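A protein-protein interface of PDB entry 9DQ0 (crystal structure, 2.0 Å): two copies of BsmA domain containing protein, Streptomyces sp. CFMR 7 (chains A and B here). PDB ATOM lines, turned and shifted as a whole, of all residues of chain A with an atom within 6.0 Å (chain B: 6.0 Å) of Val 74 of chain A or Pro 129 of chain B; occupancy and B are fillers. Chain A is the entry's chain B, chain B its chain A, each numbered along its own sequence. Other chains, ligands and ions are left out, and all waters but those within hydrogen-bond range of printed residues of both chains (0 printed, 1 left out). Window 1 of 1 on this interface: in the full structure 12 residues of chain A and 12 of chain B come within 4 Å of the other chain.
O of Tyr 32 of chain A lies close to ND2 of Asn 35 of chain B, 3.2 Å away. The side-chain amide oxygen of Asn 35 of chain B lies close to the backbone NH of Met 33 of chain A (3.2 Å).
Of chain B, only Pro 129 comes within 4 Å of Val 74 of chain A. Of the printed residues of chain A, Asn 35 of chain B touches Tyr 32 (3.1 Å) and Met 33 (3.2 Å). Of the printed residues of chain A, Val 74 of chain B touches Pro 129 (3.7 Å). Leu 127 of chain B touches none of the printed residues of chain A. The nearest residue of chain B that does not touch Val 74 of chain A is Val 74 of chain B (4.3 Å). The nearest residue of chain A that does not touch Pro 129 of chain B is Pro 73 of chain A (5.3 Å). The nearest printed residue of chain A that does not touch Asn 35 of chain B is Val 74 of chain A (4.8 Å).
The side-chain amide oxygen (OD1) of Asn 72 of chain A sits at hydrogen-bond distance from the backbone NH (N) of Val 74 of chain A (3.1 Å).
Val 74 of chain A touches Pro 129 of chain B, and with the chains exchanged Pro 129 of chain A touches Val 74 of chain B. Positions printed for both chains: 33, 74, 129 and 130. Of the 4 pairs that touch across the chains among the printed residues, 2 have their exchanged pair printed and touching as well.
Of the 11 printed residues of chain A, 4 touch a printed residue of chain B. Printed residues of chain A that touch a printed residue of chain B: Tyr 32, Met 33, Val 74 and Pro 129. Hydrophobic or aromatic side chains of chain A within 4 Å of the printed part of chain B: Val 74. Printed residues of chain B that touch a printed residue of chain A: Asn 35, Val 74 and Pro 129. Among the printed residues, no Asp or Glu carboxylate lies within 4 Å of a Lys or Arg side-chain nitrogen of the other chain.
Among the printed residues, pairs that only touch across the chains: Val 74 of chain A with Pro 129 of chain B (3.9 Å) and Pro 129 of chain A with Val 74 of chain B (3.7 Å).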
ATOM      1  N   TYR A  32     -22.909  23.030   7.757  1.00  0.00           N
ATOM      2  CA  TYR A  32     -23.862  22.043   8.241  1.00  0.00           C
ATOM      3  C   TYR A  32     -23.492  20.604   7.936  1.00  0.00           C
ATOM      4  O   TYR A  32     -24.046  19.698   8.572  1.00  0.00           O
ATOM      5  CB  TYR A  32     -25.248  22.309   7.642  1.00  0.00           C
ATOM      6  CG  TYR A  32     -25.741  23.731   7.822  1.00  0.00           C
ATOM      7  CD1 TYR A  32     -25.513  24.691   6.844  1.00  0.00           C
ATOM      8  CD2 TYR A  32     -26.441  24.106   8.970  1.00  0.00           C
ATOM      9  CE1 TYR A  32     -25.971  26.002   6.996  1.00  0.00           C
ATOM     10  CE2 TYR A  32     -26.914  25.399   9.127  1.00  0.00           C
ATOM     11  CZ  TYR A  32     -26.673  26.353   8.132  1.00  0.00           C
ATOM     12  OH  TYR A  32     -27.136  27.653   8.277  1.00  0.00           O
ATOM     13  N   MET A  33     -22.602  20.367   6.974  1.00  0.00           N
ATOM     14  CA  MET A  33     -22.290  19.022   6.511  1.00  0.00           C
ATOM     15  C   MET A  33     -20.823  18.936   6.148  1.00  0.00           C
ATOM     16  O   MET A  33     -20.260  19.886   5.608  1.00  0.00           O
ATOM     17  CB  MET A  33     -23.117  18.640   5.278  1.00  0.00           C
ATOM     18  CG  MET A  33     -24.587  18.519   5.564  1.00  0.00           C
ATOM     19  SD  MET A  33     -24.887  17.004   6.463  1.00  0.00           S
ATOM     20  CE  MET A  33     -24.892  15.831   5.092  1.00  0.00           C
ATOM     21  N   LYS A  69     -35.432  14.863   7.307  1.00  0.00           N
ATOM     22  CA  LYS A  69     -34.588  13.886   7.991  1.00  0.00           C
ATOM     23  C   LYS A  69     -34.805  12.480   7.442  1.00  0.00           C
ATOM     24  O   LYS A  69     -33.877  11.665   7.430  1.00  0.00           O
ATOM     25  CB  LYS A  69     -34.850  13.917   9.501  1.00  0.00           C
ATOM     26  CG  LYS A  69     -34.254  15.138  10.212  1.00  0.00           C
ATOM     27  CD  LYS A  69     -34.365  15.012  11.737  1.00  0.00           C
ATOM     28  CE  LYS A  69     -33.685  16.185  12.445  1.00  0.00           C
ATOM     29  NZ  LYS A  69     -33.204  15.830  13.822  1.00  0.00           N
ATOM     30  N   ASN A  72     -32.286  12.671   4.556  1.00  0.00           N
ATOM     31  CA  ASN A  72     -30.923  12.982   4.967  1.00  0.00           C
ATOM     32  C   ASN A  72     -30.955  13.157   6.479  1.00  0.00           C
ATOM     33  O   ASN A  72     -31.195  14.258   6.985  1.00  0.00           O
ATOM     34  CB  ASN A  72     -30.407  14.217   4.239  1.00  0.00           C
ATOM     35  CG  ASN A  72     -29.023  14.658   4.709  1.00  0.00           C
ATOM     36  OD1 ASN A  72     -28.432  14.069   5.614  1.00  0.00           O
ATOM     37  ND2 ASN A  72     -28.500  15.699   4.075  1.00  0.00           N
ATOM     38  N   PRO A  73     -30.722  12.081   7.233  1.00  0.00           N
ATOM     39  CA  PRO A  73     -30.791  12.191   8.698  1.00  0.00           C
ATOM     40  C   PRO A  73     -29.713  13.072   9.286  1.00  0.00           C
ATOM     41  O   PRO A  73     -29.894  13.567  10.404  1.00  0.00           O
ATOM     42  CB  PRO A  73     -30.641  10.737   9.168  1.00  0.00           C
ATOM     43  CG  PRO A  73     -30.029  10.019   8.019  1.00  0.00           C
ATOM     44  CD  PRO A  73     -30.527  10.696   6.787  1.00  0.00           C
ATOM     45  N   VAL A  74     -28.600  13.287   8.577  1.00  0.00           N
ATOM     46  CA  VAL A  74     -27.520  14.106   9.116  1.00  0.00           C
ATOM     47  C   VAL A  74     -27.779  15.590   8.871  1.00  0.00           C
ATOM     48  O   VAL A  74     -27.436  16.435   9.704  1.00  0.00           O
ATOM     49  CB  VAL A  74     -26.171  13.663   8.521  1.00  0.00           C
ATOM     50  CG1 VAL A  74     -25.069  14.584   8.988  1.00  0.00           C
ATOM     51  CG2 VAL A  74     -25.858  12.229   8.939  1.00  0.00           C
ATOM     52  N   GLY A  75     -28.362  15.942   7.730  1.00  0.00           N
ATOM     53  CA  GLY A  75     -28.515  17.349   7.398  1.00  0.00           C
ATOM     54  C   GLY A  75     -29.939  17.811   7.152  1.00  0.00           C
ATOM     55  O   GLY A  75     -30.167  18.919   6.651  1.00  0.00           O
ATOM     56  N   GLY A  76     -30.909  16.964   7.491  1.00  0.00           N
ATOM     57  CA  GLY A  76     -32.301  17.290   7.256  1.00  0.00           C
ATOM     58  C   GLY A  76     -32.939  17.985   8.434  1.00  0.00           C
ATOM     59  O   GLY A  76     -32.362  18.068   9.526  1.00  0.00           O
ATOM     60  N   ILE A  78     -33.459  21.047   9.100  1.00  0.00           N
ATOM     61  CA  ILE A  78     -32.949  22.338   9.550  1.00  0.00           C
ATOM     62  C   ILE A  78     -32.870  23.296   8.371  1.00  0.00           C
ATOM     63  O   ILE A  78     -32.755  22.883   7.213  1.00  0.00           O
ATOM     64  CB  ILE A  78     -31.567  22.226  10.238  1.00  0.00           C
ATOM     65  CG1 ILE A  78     -30.531  21.620   9.291  1.00  0.00           C
ATOM     66  CG2 ILE A  78     -31.668  21.402  11.505  1.00  0.00           C
ATOM     67  CD1 ILE A  78     -29.125  21.759   9.782  1.00  0.00           C
ATOM     68  N   PRO A 129     -22.295  11.237   4.058  1.00  0.00           N
ATOM     69  CA  PRO A 129     -22.297  10.771   5.452  1.00  0.00           C
ATOM     70  C   PRO A 129     -23.651  10.275   5.894  1.00  0.00           C
ATOM     71  O   PRO A 129     -23.731   9.469   6.820  1.00  0.00           O
ATOM     72  CB  PRO A 129     -21.858  12.011   6.245  1.00  0.00           C
ATOM     73  CG  PRO A 129     -22.127  13.169   5.355  1.00  0.00           C
ATOM     74  CD  PRO A 129     -21.917  12.659   3.956  1.00  0.00           C
ATOM     75  N   GLU A 130     -24.718  10.694   5.229  1.00  0.00           N
ATOM     76  CA  GLU A 130     -26.027  10.122   5.491  1.00  0.00           C
ATOM     77  C   GLU A 130     -26.109   8.647   5.085  1.00  0.00           C
ATOM     78  O   GLU A 130     -27.057   7.957   5.474  1.00  0.00           O
ATOM     79  CB  GLU A 130     -27.095  10.952   4.760  1.00  0.00           C
ATOM     80  CG  GLU A 130     -27.031  10.943   3.212  1.00  0.00           C
ATOM     81  CD  GLU A 130     -26.136  12.037   2.613  1.00  0.00           C
ATOM     82  OE1 GLU A 130     -25.124  12.426   3.235  1.00  0.00           O
ATOM     83  OE2 GLU A 130     -26.445  12.518   1.508  1.00  0.00           O
ATOM     84  N   MET B  33     -16.963  15.719  14.088  1.00  0.00           N
ATOM     85  CA  MET B  33     -18.377  15.416  14.270  1.00  0.00           C
ATOM     86  C   MET B  33     -19.106  16.664  14.723  1.00  0.00           C
ATOM     87  O   MET B  33     -18.543  17.481  15.454  1.00  0.00           O
ATOM     88  CB  MET B  33     -18.588  14.331  15.322  1.00  0.00           C
ATOM     89  CG  MET B  33     -17.581  13.207  15.261  1.00  0.00           C
ATOM     90  SD  MET B  33     -18.405  11.618  15.400  1.00  0.00           S
ATOM     91  CE  MET B  33     -19.410  11.716  13.931  1.00  0.00           C
ATOM     92  N   GLY B  34     -20.364  16.795  14.307  1.00  0.00           N
ATOM     93  CA  GLY B  34     -21.233  17.821  14.844  1.00  0.00           C
ATOM     94  C   GLY B  34     -21.237  19.120  14.082  1.00  0.00           C
ATOM     95  O   GLY B  34     -22.016  20.018  14.433  1.00  0.00           O
ATOM     96  N   ASN B  35     -20.379  19.260  13.071  1.00  0.00           N
ATOM     97  CA  ASN B  35     -20.420  20.404  12.174  1.00  0.00           C
ATOM     98  C   ASN B  35     -20.415  21.715  12.948  1.00  0.00           C
ATOM     99  O   ASN B  35     -21.240  22.607  12.729  1.00  0.00           O
ATOM    100  CB  ASN B  35     -21.627  20.282  11.253  1.00  0.00           C
ATOM    101  CG  ASN B  35     -21.423  19.196  10.230  1.00  0.00           C
ATOM    102  OD1 ASN B  35     -20.654  19.386   9.281  1.00  0.00           O
ATOM    103  ND2 ASN B  35     -22.047  18.031  10.440  1.00  0.00           N
ATOM    104  N   ARG B  38     -20.141  20.785  18.298  1.00  0.00           N
ATOM    105  CA  ARG B  38     -19.623  19.888  19.316  1.00  0.00           C
ATOM    106  C   ARG B  38     -18.201  20.277  19.691  1.00  0.00           C
ATOM    107  O   ARG B  38     -17.411  20.704  18.839  1.00  0.00           O
ATOM    108  CB  ARG B  38     -19.654  18.434  18.844  1.00  0.00           C
ATOM    109  CG  ARG B  38     -19.268  17.433  19.933  1.00  0.00           C
ATOM    110  CD  ARG B  38     -19.503  15.994  19.514  1.00  0.00           C
ATOM    111  NE  ARG B  38     -20.885  15.719  19.152  1.00  0.00           N
ATOM    112  CZ  ARG B  38     -21.303  14.537  18.725  1.00  0.00           C
ATOM    113  NH1 ARG B  38     -20.479  13.505  18.652  1.00  0.00           N
ATOM    114  NH2 ARG B  38     -22.573  14.389  18.357  1.00  0.00           N
ATOM    115  N   VAL B  74     -20.506   7.837  10.551  1.00  0.00           N
ATOM    116  CA  VAL B  74     -20.197   9.233  10.280  1.00  0.00           C
ATOM    117  C   VAL B  74     -18.783   9.583  10.749  1.00  0.00           C
ATOM    118  O   VAL B  74     -18.087  10.383  10.116  1.00  0.00           O
ATOM    119  CB  VAL B  74     -21.268  10.122  10.946  1.00  0.00           C
ATOM    120  CG1 VAL B  74     -20.941  11.567  10.760  1.00  0.00           C
ATOM    121  CG2 VAL B  74     -22.608   9.823  10.357  1.00  0.00           C
ATOM    122  N   PRO B 126     -26.778  18.120  17.240  1.00  0.00           N
ATOM    123  CA  PRO B 126     -26.893  16.665  17.040  1.00  0.00           C
ATOM    124  C   PRO B 126     -26.024  15.902  18.030  1.00  0.00           C
ATOM    125  O   PRO B 126     -24.840  16.192  18.193  1.00  0.00           O
ATOM    126  CB  PRO B 126     -26.418  16.462  15.596  1.00  0.00           C
ATOM    127  CG  PRO B 126     -26.419  17.827  14.966  1.00  0.00           C
ATOM    128  CD  PRO B 126     -26.125  18.779  16.095  1.00  0.00           C
ATOM    129  N   LEU B 127     -26.626  14.928  18.694  1.00  0.00           N
ATOM    130  CA  LEU B 127     -25.929  14.084  19.661  1.00  0.00           C
ATOM    131  C   LEU B 127     -25.514  12.735  19.086  1.00  0.00           C
ATOM    132  O   LEU B 127     -24.412  12.256  19.374  1.00  0.00           O
ATOM    133  CB  LEU B 127     -26.813  13.873  20.886  1.00  0.00           C
ATOM    134  CG  LEU B 127     -27.078  15.161  21.663  1.00  0.00           C
ATOM    135  CD1 LEU B 127     -28.079  14.925  22.776  1.00  0.00           C
ATOM    136  CD2 LEU B 127     -25.750  15.742  22.226  1.00  0.00           C
ATOM    137  N   THR B 128     -26.361  12.101  18.270  1.00  0.00           N
ATOM    138  CA  THR B 128     -26.027  10.835  17.631  1.00  0.00           C
ATOM    139  C   THR B 128     -26.370  10.932  16.149  1.00  0.00           C
ATOM    140  O   THR B 128     -27.290  10.266  15.663  1.00  0.00           O
ATOM    141  CB  THR B 128     -26.761   9.669  18.300  1.00  0.00           C
ATOM    142  OG1 THR B 128     -28.164   9.900  18.207  1.00  0.00           O
ATOM    143  CG2 THR B 128     -26.409   9.574  19.792  1.00  0.00           C
ATOM    144  N   PRO B 129     -25.640  11.752  15.391  1.00  0.00           N
ATOM    145  CA  PRO B 129     -25.884  11.791  13.948  1.00  0.00           C
ATOM    146  C   PRO B 129     -25.648  10.451  13.292  1.00  0.00           C
ATOM    147  O   PRO B 129     -26.181  10.216  12.208  1.00  0.00           O
ATOM    148  CB  PRO B 129     -24.888  12.847  13.454  1.00  0.00           C
ATOM    149  CG  PRO B 129     -23.796  12.789  14.436  1.00  0.00           C
ATOM    150  CD  PRO B 129     -24.488  12.592  15.754  1.00  0.00           C
ATOM    151  N   GLU B 130     -24.881   9.557  13.920  1.00  0.00           N
ATOM    152  CA  GLU B 130     -24.787   8.192  13.422  1.00  0.00           C
ATOM    153  C   GLU B 130     -26.128   7.457  13.477  1.00  0.00           C
ATOM    154  O   GLU B 130     -26.271   6.402  12.849  1.00  0.00           O
ATOM    155  CB  GLU B 130     -23.719   7.414  14.212  1.00  0.00           C
ATOM    156  CG  GLU B 130     -23.978   7.192  15.704  1.00  0.00           C
ATOM    157  CD  GLU B 130     -23.470   8.337  16.572  1.00  0.00           C
ATOM    158  OE1 GLU B 130     -23.528   9.508  16.129  1.00  0.00           O
ATOM    159  OE2 GLU B 130     -23.005   8.069  17.692  1.00  0.00           O
ATOM    160  N   GLY B 131     -27.109   7.977  14.211  1.00  0.00           N
ATOM    161  CA  GLY B 131     -28.392   7.302  14.360  1.00  0.00           C
ATOM    162  C   GLY B 131     -28.360   6.201  15.414  1.00  0.00           C
ATOM    163  O   GLY B 131     -27.481   6.151  16.287  1.00  0.00           O
